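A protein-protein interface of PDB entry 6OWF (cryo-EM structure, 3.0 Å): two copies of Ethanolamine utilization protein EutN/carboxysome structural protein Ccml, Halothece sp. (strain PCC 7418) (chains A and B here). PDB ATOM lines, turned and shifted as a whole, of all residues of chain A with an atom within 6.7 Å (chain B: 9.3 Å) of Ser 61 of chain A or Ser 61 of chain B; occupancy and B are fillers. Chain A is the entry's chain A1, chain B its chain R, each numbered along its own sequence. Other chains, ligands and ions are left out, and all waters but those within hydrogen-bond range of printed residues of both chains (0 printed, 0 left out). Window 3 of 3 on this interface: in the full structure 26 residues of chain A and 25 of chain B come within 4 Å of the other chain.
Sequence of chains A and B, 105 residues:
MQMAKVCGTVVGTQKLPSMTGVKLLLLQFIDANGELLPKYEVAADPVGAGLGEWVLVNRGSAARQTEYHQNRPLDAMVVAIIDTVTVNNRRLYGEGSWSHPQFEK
Printed residues of chain A that touch a printed residue of chain B: Asn 58, Arg 59, Ser 61, Ala 62 and Gln 65.
Along chain A the printed residues that touch a printed residue of chain B span positions 58 to 65.
Hydrophobic or aromatic side chains of chain B that line the printed part of chain A: Pro 73.
Among the printed residues, 12 pairs touch across the chains.
Among the printed residues, no Asp or Glu carboxylate lies within 4 Å of a Lys or Arg side-chain nitrogen of the other chain.
Asn 58 of chain A touches Asp 75 of chain B, but with the chains exchanged Asp 75 of chain A does not touch Asn 58 of chain B (14.1 Å).
Arg 59 of chain A touches its own counterpart, Arg 59 of chain B.
Ser 61 of chain A touches Arg 64 of chain B, but with the chains exchanged Arg 64 of chain A does not touch Ser 61 of chain B (7.6 Å).
Ala 62 of chain A touches Leu 74 of chain B, but with the chains exchanged Leu 74 of chain A does not touch Ala 62 of chain B (14.0 Å).
Of the 12 pairs that touch across the chains among the printed residues, 2 have their exchanged pair printed and touching as well.
Ser 61 of chain A touches just these residues of chain B: Ser 61 (3.6 Å) and Arg 64 (2.7 Å).
Ser 61 of chain B touches one residue of chain A.
No residue of chain B comes within 4 Å of Gly 60 of chain A.
No residue of chain B comes within 4 Å of Arg 64 of chain A.
Of the printed residues of chain A, Arg 59 of chain B touches Arg 59 (3.5 Å).
Printed residues of chain B within 4 Å of Asn 58 of chain A: Pro 73 (2.9 Å) and Asp 75 (3.3 Å).
Of the printed residues of chain A, Asp 75 of chain B touches Asn 58 and Arg 59.
Thr 66 of chain B touches none of the printed residues of chain A.
Ala 63 of chain B touches none of the printed residues of chain A.
The nearest residue of chain B that does not touch Ser 61 of chain A is Gly 60 of chain B (5.3 Å).
The nearest printed residue of chain A that does not touch Arg 59 of chain B is Gly 60 of chain A (7.7 Å).
O of Ser 61 of chain A lies within hydrogen-bond range of NE2 of Gln 65 of chain A, 3.2 Å away.
The side-chain amide nitrogen of Gln 65 of chain B lies within hydrogen-bond range of the backbone carbonyl oxygen of Ser 61 of chain B (3.3 Å).
N of Gly 60 of chain B lies within hydrogen-bond range of O of Asp 75 of chain B (2.9 Å).
The side-chain amide nitrogen (ND2) of Asn 58 of chain A lies close to the backbone carbonyl oxygen (O) of Ala 62 of chain A (3.4 Å).
The guanidinium group of Arg 64 of chain B sits at hydrogen-bond distance from the side-chain hydroxyl of Ser 61 of chain A, 2.7 Å away.
The backbone carbonyl oxygen (O) of Asn 71 of chain B lies close to the backbone carbonyl oxygen (O) of Gln 65 of chain A, at 3.4 Å.
N of Arg 59 of chain A lies within hydrogen-bond range of OD2 of Asp 75 of chain B.
The backbone carbonyl oxygen (O) of Pro 73 of chain B is in hydrogen-bond range of the side-chain amide nitrogen (ND2) of Asn 58 of chain A, 2.9 Å away.
NE2 of Gln 65 of chain A sits close to NH1 of Arg 64 of chain B (3.3 Å).
Asn 58 of chain A touches Asp 75 of chain B.
NH2 of Arg 59 of chain B touches CD of Arg 59 of chain A, at 3.5 Å.
Ser 61 of chain A touches Ser 61 of chain B.
Arg 64 of chain B touches Ala 62 of chain A.
O of Ala 62 of chain A touches CB of Pro 73 of chain B (3.3 Å).
Leu 74 of chain B touches Ala 62 of chain A (O to CB, 3.4 Å).
Gln 65 of chain A touches Gln 70 of chain B (OE1 to O, 3.8 Å).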
ATOM      1  N   ASN A  58      -4.074  14.225   6.500  1.00  0.00           N
ATOM      2  CA  ASN A  58      -5.196  14.273   7.422  1.00  0.00           C
ATOM      3  C   ASN A  58      -4.682  14.223   8.852  1.00  0.00           C
ATOM      4  O   ASN A  58      -3.672  13.583   9.141  1.00  0.00           O
ATOM      5  CB  ASN A  58      -6.178  13.125   7.174  1.00  0.00           C
ATOM      6  CG  ASN A  58      -5.541  11.765   7.307  1.00  0.00           C
ATOM      7  OD1 ASN A  58      -4.336  11.616   7.173  1.00  0.00           O
ATOM      8  ND2 ASN A  58      -6.356  10.755   7.552  1.00  0.00           N
ATOM      9  N   ARG A  59      -5.379  14.911   9.747  1.00  0.00           N
ATOM     10  CA  ARG A  59      -4.955  15.011  11.133  1.00  0.00           C
ATOM     11  C   ARG A  59      -5.918  14.264  12.044  1.00  0.00           C
ATOM     12  O   ARG A  59      -7.093  14.080  11.722  1.00  0.00           O
ATOM     13  CB  ARG A  59      -4.850  16.474  11.571  1.00  0.00           C
ATOM     14  CG  ARG A  59      -6.152  17.247  11.511  1.00  0.00           C
ATOM     15  CD  ARG A  59      -5.919  18.737  11.702  1.00  0.00           C
ATOM     16  NE  ARG A  59      -4.805  19.005  12.607  1.00  0.00           N
ATOM     17  CZ  ARG A  59      -4.942  19.298  13.894  1.00  0.00           C
ATOM     18  NH1 ARG A  59      -6.149  19.368  14.439  1.00  0.00           N
ATOM     19  NH2 ARG A  59      -3.869  19.524  14.640  1.00  0.00           N
ATOM     20  N   GLY A  60      -5.401  13.821  13.176  1.00  0.00           N
ATOM     21  CA  GLY A  60      -6.214  13.270  14.238  1.00  0.00           C
ATOM     22  C   GLY A  60      -6.199  11.754  14.255  1.00  0.00           C
ATOM     23  O   GLY A  60      -5.223  11.100  13.881  1.00  0.00           O
ATOM     24  N   SER A  61      -7.327  11.196  14.699  1.00  0.00           N
ATOM     25  CA  SER A  61      -7.483   9.751  14.807  1.00  0.00           C
ATOM     26  C   SER A  61      -7.657   9.074  13.460  1.00  0.00           C
ATOM     27  O   SER A  61      -7.614   7.841  13.395  1.00  0.00           O
ATOM     28  CB  SER A  61      -8.679   9.421  15.697  1.00  0.00           C
ATOM     29  OG  SER A  61      -9.889   9.819  15.085  1.00  0.00           O
ATOM     30  N   ALA A  62      -7.853   9.842  12.388  1.00  0.00           N
ATOM     31  CA  ALA A  62      -7.975   9.272  11.055  1.00  0.00           C
ATOM     32  C   ALA A  62      -6.651   8.744  10.528  1.00  0.00           C
ATOM     33  O   ALA A  62      -6.645   7.976   9.564  1.00  0.00           O
ATOM     34  CB  ALA A  62      -8.543  10.315  10.098  1.00  0.00           C
ATOM     35  N   ALA A  63      -5.532   9.125  11.147  1.00  0.00           N
ATOM     36  CA  ALA A  63      -4.229   8.607  10.755  1.00  0.00           C
ATOM     37  C   ALA A  63      -3.990   7.183  11.240  1.00  0.00           C
ATOM     38  O   ALA A  63      -2.963   6.592  10.897  1.00  0.00           O
ATOM     39  CB  ALA A  63      -3.131   9.520  11.291  1.00  0.00           C
ATOM     40  N   ARG A  64      -4.903   6.621  12.031  1.00  0.00           N
ATOM     41  CA  ARG A  64      -4.751   5.292  12.602  1.00  0.00           C
ATOM     42  C   ARG A  64      -5.801   4.314  12.095  1.00  0.00           C
ATOM     43  O   ARG A  64      -6.303   3.498  12.874  1.00  0.00           O
ATOM     44  CB  ARG A  64      -4.807   5.376  14.126  1.00  0.00           C
ATOM     45  CG  ARG A  64      -3.938   6.465  14.702  1.00  0.00           C
ATOM     46  CD  ARG A  64      -3.924   6.421  16.206  1.00  0.00           C
ATOM     47  NE  ARG A  64      -5.024   7.171  16.795  1.00  0.00           N
ATOM     48  CZ  ARG A  64      -6.106   6.611  17.318  1.00  0.00           C
ATOM     49  NH1 ARG A  64      -6.236   5.293  17.321  1.00  0.00           N
ATOM     50  NH2 ARG A  64      -7.059   7.366  17.841  1.00  0.00           N
ATOM     51  N   GLN A  65      -6.147   4.375  10.813  1.00  0.00           N
ATOM     52  CA  GLN A  65      -7.247   3.587  10.275  1.00  0.00           C
ATOM     53  C   GLN A  65      -6.838   2.653   9.145  1.00  0.00           C
ATOM     54  O   GLN A  65      -7.716   2.121   8.462  1.00  0.00           O
ATOM     55  CB  GLN A  65      -8.364   4.511   9.781  1.00  0.00           C
ATOM     56  CG  GLN A  65      -8.940   5.426  10.839  1.00  0.00           C
ATOM     57  CD  GLN A  65      -9.570   4.668  11.986  1.00  0.00           C
ATOM     58  OE1 GLN A  65     -10.222   3.645  11.786  1.00  0.00           O
ATOM     59  NE2 GLN A  65      -9.380   5.168  13.200  1.00  0.00           N
ATOM     60  N   LEU A  74       0.082   7.978  16.016  1.00  0.00           N
ATOM     61  CA  LEU A  74       0.138   8.877  14.873  1.00  0.00           C
ATOM     62  C   LEU A  74      -1.078   9.787  14.872  1.00  0.00           C
ATOM     63  O   LEU A  74      -2.210   9.318  15.024  1.00  0.00           O
ATOM     64  CB  LEU A  74       0.192   8.096  13.562  1.00  0.00           C
ATOM     65  CG  LEU A  74       1.361   7.138  13.386  1.00  0.00           C
ATOM     66  CD1 LEU A  74       1.246   6.471  12.050  1.00  0.00           C
ATOM     67  CD2 LEU A  74       2.664   7.885  13.485  1.00  0.00           C
ATOM     68  N   ASP A  75      -0.843  11.084  14.691  1.00  0.00           N
ATOM     69  CA  ASP A  75      -1.920  12.052  14.552  1.00  0.00           C
ATOM     70  C   ASP A  75      -1.861  12.779  13.217  1.00  0.00           C
ATOM     71  O   ASP A  75      -2.533  13.802  13.051  1.00  0.00           O
ATOM     72  CB  ASP A  75      -1.889  13.058  15.706  1.00  0.00           C
ATOM     73  CG  ASP A  75      -0.746  14.039  15.591  1.00  0.00           C
ATOM     74  OD1 ASP A  75       0.368  13.606  15.249  1.00  0.00           O
ATOM     75  OD2 ASP A  75      -0.965  15.246  15.835  1.00  0.00           O
ATOM     76  N   ASN B  58     -17.842  18.783   8.680  1.00  0.00           N
ATOM     77  CA  ASN B  58     -17.434  18.452  10.034  1.00  0.00           C
ATOM     78  C   ASN B  58     -16.029  17.872  10.017  1.00  0.00           C
ATOM     79  O   ASN B  58     -15.654  17.145   9.097  1.00  0.00           O
ATOM     80  CB  ASN B  58     -18.400  17.460  10.687  1.00  0.00           C
ATOM     81  CG  ASN B  58     -18.576  16.198   9.883  1.00  0.00           C
ATOM     82  OD1 ASN B  58     -18.305  16.166   8.694  1.00  0.00           O
ATOM     83  ND2 ASN B  58     -19.052  15.149  10.530  1.00  0.00           N
ATOM     84  N   ARG B  59     -15.251  18.202  11.038  1.00  0.00           N
ATOM     85  CA  ARG B  59     -13.871  17.757  11.126  1.00  0.00           C
ATOM     86  C   ARG B  59     -13.722  16.695  12.205  1.00  0.00           C
ATOM     87  O   ARG B  59     -14.489  16.652  13.169  1.00  0.00           O
ATOM     88  CB  ARG B  59     -12.928  18.928  11.417  1.00  0.00           C
ATOM     89  CG  ARG B  59     -13.228  19.682  12.698  1.00  0.00           C
ATOM     90  CD  ARG B  59     -12.451  20.986  12.760  1.00  0.00           C
ATOM     91  NE  ARG B  59     -11.144  20.868  12.122  1.00  0.00           N
ATOM     92  CZ  ARG B  59     -10.007  20.661  12.776  1.00  0.00           C
ATOM     93  NH1 ARG B  59     -10.008  20.554  14.097  1.00  0.00           N
ATOM     94  NH2 ARG B  59      -8.867  20.563  12.108  1.00  0.00           N
ATOM     95  N   GLY B  60     -12.742  15.829  12.023  1.00  0.00           N
ATOM     96  CA  GLY B  60     -12.345  14.887  13.044  1.00  0.00           C
ATOM     97  C   GLY B  60     -12.854  13.486  12.773  1.00  0.00           C
ATOM     98  O   GLY B  60     -13.038  13.060  11.632  1.00  0.00           O
ATOM     99  N   SER B  61     -13.091  12.763  13.870  1.00  0.00           N
ATOM    100  CA  SER B  61     -13.551  11.383  13.808  1.00  0.00           C
ATOM    101  C   SER B  61     -15.011  11.262  13.406  1.00  0.00           C
ATOM    102  O   SER B  61     -15.476  10.146  13.154  1.00  0.00           O
ATOM    103  CB  SER B  61     -13.340  10.705  15.160  1.00  0.00           C
ATOM    104  OG  SER B  61     -13.927  11.460  16.200  1.00  0.00           O
ATOM    105  N   ALA B  62     -15.743  12.374  13.344  1.00  0.00           N
ATOM    106  CA  ALA B  62     -17.133  12.340  12.919  1.00  0.00           C
ATOM    107  C   ALA B  62     -17.273  12.088  11.426  1.00  0.00           C
ATOM    108  O   ALA B  62     -18.362  11.726  10.973  1.00  0.00           O
ATOM    109  CB  ALA B  62     -17.820  13.647  13.296  1.00  0.00           C
ATOM    110  N   ALA B  63     -16.198  12.257  10.656  1.00  0.00           N
ATOM    111  CA  ALA B  63     -16.228  11.948   9.233  1.00  0.00           C
ATOM    112  C   ALA B  63     -16.188  10.450   8.959  1.00  0.00           C
ATOM    113  O   ALA B  63     -16.367  10.040   7.809  1.00  0.00           O
ATOM    114  CB  ALA B  63     -15.060  12.631   8.528  1.00  0.00           C
ATOM    115  N   ARG B  64     -15.955   9.627   9.980  1.00  0.00           N
ATOM    116  CA  ARG B  64     -15.880   8.182   9.837  1.00  0.00           C
ATOM    117  C   ARG B  64     -17.043   7.467  10.508  1.00  0.00           C
ATOM    118  O   ARG B  64     -16.850   6.397  11.090  1.00  0.00           O
ATOM    119  CB  ARG B  64     -14.558   7.672  10.406  1.00  0.00           C
ATOM    120  CG  ARG B  64     -13.365   8.482   9.976  1.00  0.00           C
ATOM    121  CD  ARG B  64     -12.084   7.871  10.474  1.00  0.00           C
ATOM    122  NE  ARG B  64     -11.748   8.307  11.822  1.00  0.00           N
ATOM    123  CZ  ARG B  64     -11.918   7.561  12.905  1.00  0.00           C
ATOM    124  NH1 ARG B  64     -12.427   6.343  12.798  1.00  0.00           N
ATOM    125  NH2 ARG B  64     -11.580   8.030  14.094  1.00  0.00           N
ATOM    126  N   GLN B  65     -18.244   8.033  10.444  1.00  0.00           N
ATOM    127  CA  GLN B  65     -19.393   7.491  11.151  1.00  0.00           C
ATOM    128  C   GLN B  65     -20.549   7.129  10.231  1.00  0.00           C
ATOM    129  O   GLN B  65     -21.685   7.039  10.702  1.00  0.00           O
ATOM    130  CB  GLN B  65     -19.883   8.491  12.202  1.00  0.00           C
ATOM    131  CG  GLN B  65     -18.858   8.853  13.255  1.00  0.00           C
ATOM    132  CD  GLN B  65     -18.433   7.666  14.088  1.00  0.00           C
ATOM    133  OE1 GLN B  65     -19.243   6.801  14.416  1.00  0.00           O
ATOM    134  NE2 GLN B  65     -17.155   7.620  14.440  1.00  0.00           N
ATOM    135  N   THR B  66     -20.302   6.931   8.938  1.00  0.00           N
ATOM    136  CA  THR B  66     -21.382   6.825   7.969  1.00  0.00           C
ATOM    137  C   THR B  66     -21.350   5.542   7.153  1.00  0.00           C
ATOM    138  O   THR B  66     -21.425   5.619   5.922  1.00  0.00           O
ATOM    139  CB  THR B  66     -21.361   8.027   7.026  1.00  0.00           C
ATOM    140  OG1 THR B  66     -20.014   8.295   6.623  1.00  0.00           O
ATOM    141  CG2 THR B  66     -21.929   9.246   7.717  1.00  0.00           C
ATOM    142  N   HIS B  69     -17.535   4.982   5.432  1.00  0.00           N
ATOM    143  CA  HIS B  69     -16.347   5.758   5.737  1.00  0.00           C
ATOM    144  C   HIS B  69     -15.688   5.311   7.034  1.00  0.00           C
ATOM    145  O   HIS B  69     -14.826   6.023   7.553  1.00  0.00           O
ATOM    146  CB  HIS B  69     -16.701   7.243   5.817  1.00  0.00           C
ATOM    147  CG  HIS B  69     -16.903   7.892   4.484  1.00  0.00           C
ATOM    148  ND1 HIS B  69     -17.338   9.192   4.349  1.00  0.00           N
ATOM    149  CD2 HIS B  69     -16.704   7.430   3.228  1.00  0.00           C
ATOM    150  CE1 HIS B  69     -17.412   9.498   3.067  1.00  0.00           C
ATOM    151  NE2 HIS B  69     -17.034   8.447   2.365  1.00  0.00           N
ATOM    152  N   GLN B  70     -16.065   4.139   7.552  1.00  0.00           N
ATOM    153  CA  GLN B  70     -15.678   3.748   8.906  1.00  0.00           C
ATOM    154  C   GLN B  70     -14.195   3.417   9.007  1.00  0.00           C
ATOM    155  O   GLN B  70     -13.526   3.829   9.961  1.00  0.00           O
ATOM    156  CB  GLN B  70     -16.513   2.555   9.359  1.00  0.00           C
ATOM    157  CG  GLN B  70     -17.783   2.929  10.080  1.00  0.00           C
ATOM    158  CD  GLN B  70     -18.583   1.717  10.491  1.00  0.00           C
ATOM    159  OE1 GLN B  70     -18.496   0.663   9.861  1.00  0.00           O
ATOM    160  NE2 GLN B  70     -19.369   1.855  11.552  1.00  0.00           N
ATOM    161  N   ASN B  71     -13.663   2.675   8.043  1.00  0.00           N
ATOM    162  CA  ASN B  71     -12.264   2.278   8.052  1.00  0.00           C
ATOM    163  C   ASN B  71     -11.454   3.043   7.012  1.00  0.00           C
ATOM    164  O   ASN B  71     -10.453   2.539   6.500  1.00  0.00           O
ATOM    165  CB  ASN B  71     -12.141   0.773   7.832  1.00  0.00           C
ATOM    166  CG  ASN B  71     -13.006  -0.022   8.784  1.00  0.00           C
ATOM    167  OD1 ASN B  71     -12.990   0.206   9.992  1.00  0.00           O
ATOM    168  ND2 ASN B  71     -13.779  -0.956   8.243  1.00  0.00           N
ATOM    169  N   ARG B  72     -11.877   4.242   6.696  1.00  0.00           N
ATOM    170  CA  ARG B  72     -11.192   5.128   5.776  1.00  0.00           C
ATOM    171  C   ARG B  72     -10.499   6.250   6.536  1.00  0.00           C
ATOM    172  O   ARG B  72     -10.999   6.711   7.564  1.00  0.00           O
ATOM    173  CB  ARG B  72     -12.176   5.726   4.767  1.00  0.00           C
ATOM    174  CG  ARG B  72     -12.886   4.695   3.917  1.00  0.00           C
ATOM    175  CD  ARG B  72     -13.678   5.359   2.814  1.00  0.00           C
ATOM    176  NE  ARG B  72     -14.599   4.432   2.167  1.00  0.00           N
ATOM    177  CZ  ARG B  72     -14.310   3.731   1.077  1.00  0.00           C
ATOM    178  NH1 ARG B  72     -15.210   2.910   0.555  1.00  0.00           N
ATOM    179  NH2 ARG B  72     -13.121   3.852   0.505  1.00  0.00           N
ATOM    180  N   PRO B  73      -9.342   6.704   6.070  1.00  0.00           N
ATOM    181  CA  PRO B  73      -8.628   7.787   6.776  1.00  0.00           C
ATOM    182  C   PRO B  73      -9.140   9.174   6.407  1.00  0.00           C
ATOM    183  O   PRO B  73      -8.498   9.960   5.708  1.00  0.00           O
ATOM    184  CB  PRO B  73      -7.180   7.557   6.335  1.00  0.00           C
ATOM    185  CG  PRO B  73      -7.295   6.956   4.997  1.00  0.00           C
ATOM    186  CD  PRO B  73      -8.518   6.101   5.011  1.00  0.00           C
ATOM    187  N   LEU B  74     -10.329   9.504   6.900  1.00  0.00           N
ATOM    188  CA  LEU B  74     -10.980  10.772   6.605  1.00  0.00           C
ATOM    189  C   LEU B  74     -11.118  11.588   7.879  1.00  0.00           C
ATOM    190  O   LEU B  74     -11.590  11.077   8.899  1.00  0.00           O
ATOM    191  CB  LEU B  74     -12.357  10.550   5.986  1.00  0.00           C
ATOM    192  CG  LEU B  74     -12.393   9.735   4.702  1.00  0.00           C
ATOM    193  CD1 LEU B  74     -13.819   9.536   4.293  1.00  0.00           C
ATOM    194  CD2 LEU B  74     -11.632  10.440   3.610  1.00  0.00           C
ATOM    195  N   ASP B  75     -10.716  12.854   7.817  1.00  0.00           N
ATOM    196  CA  ASP B  75     -10.919  13.775   8.925  1.00  0.00           C
ATOM    197  C   ASP B  75     -11.792  14.956   8.530  1.00  0.00           C
ATOM    198  O   ASP B  75     -11.812  15.965   9.242  1.00  0.00           O
ATOM    199  CB  ASP B  75      -9.575  14.265   9.476  1.00  0.00           C
ATOM    200  CG  ASP B  75      -8.876  15.227   8.543  1.00  0.00           C
ATOM    201  OD1 ASP B  75      -8.908  14.995   7.323  1.00  0.00           O
ATOM    202  OD2 ASP B  75      -8.296  16.218   9.030  1.00  0.00           O
ATOM    203  N   ALA B  76     -12.512  14.855   7.415  1.00  0.00           N
ATOM    204  CA  ALA B  76     -13.449  15.883   6.988  1.00  0.00           C
ATOM    205  C   ALA B  76     -14.458  15.249   6.048  1.00  0.00           C
ATOM    206  O   ALA B  76     -14.101  14.393   5.239  1.00  0.00           O
ATOM    207  CB  ALA B  76     -12.739  17.047   6.295  1.00  0.00           C
ATOM    208  N   MET B  77     -15.712  15.673   6.159  1.00  0.00           N
ATOM    209  CA  MET B  77     -16.779  15.138   5.329  1.00  0.00           C
ATOM    210  C   MET B  77     -17.839  16.209   5.156  1.00  0.00           C
ATOM    211  O   MET B  77     -17.998  17.076   6.010  1.00  0.00           O
ATOM    212  CB  MET B  77     -17.398  13.885   5.946  1.00  0.00           C
ATOM    213  CG  MET B  77     -17.962  12.907   4.945  1.00  0.00           C
ATOM    214  SD  MET B  77     -18.661  11.440   5.718  1.00  0.00           S
ATOM    215  CE  MET B  77     -19.586  12.176   7.056  1.00  0.00           C
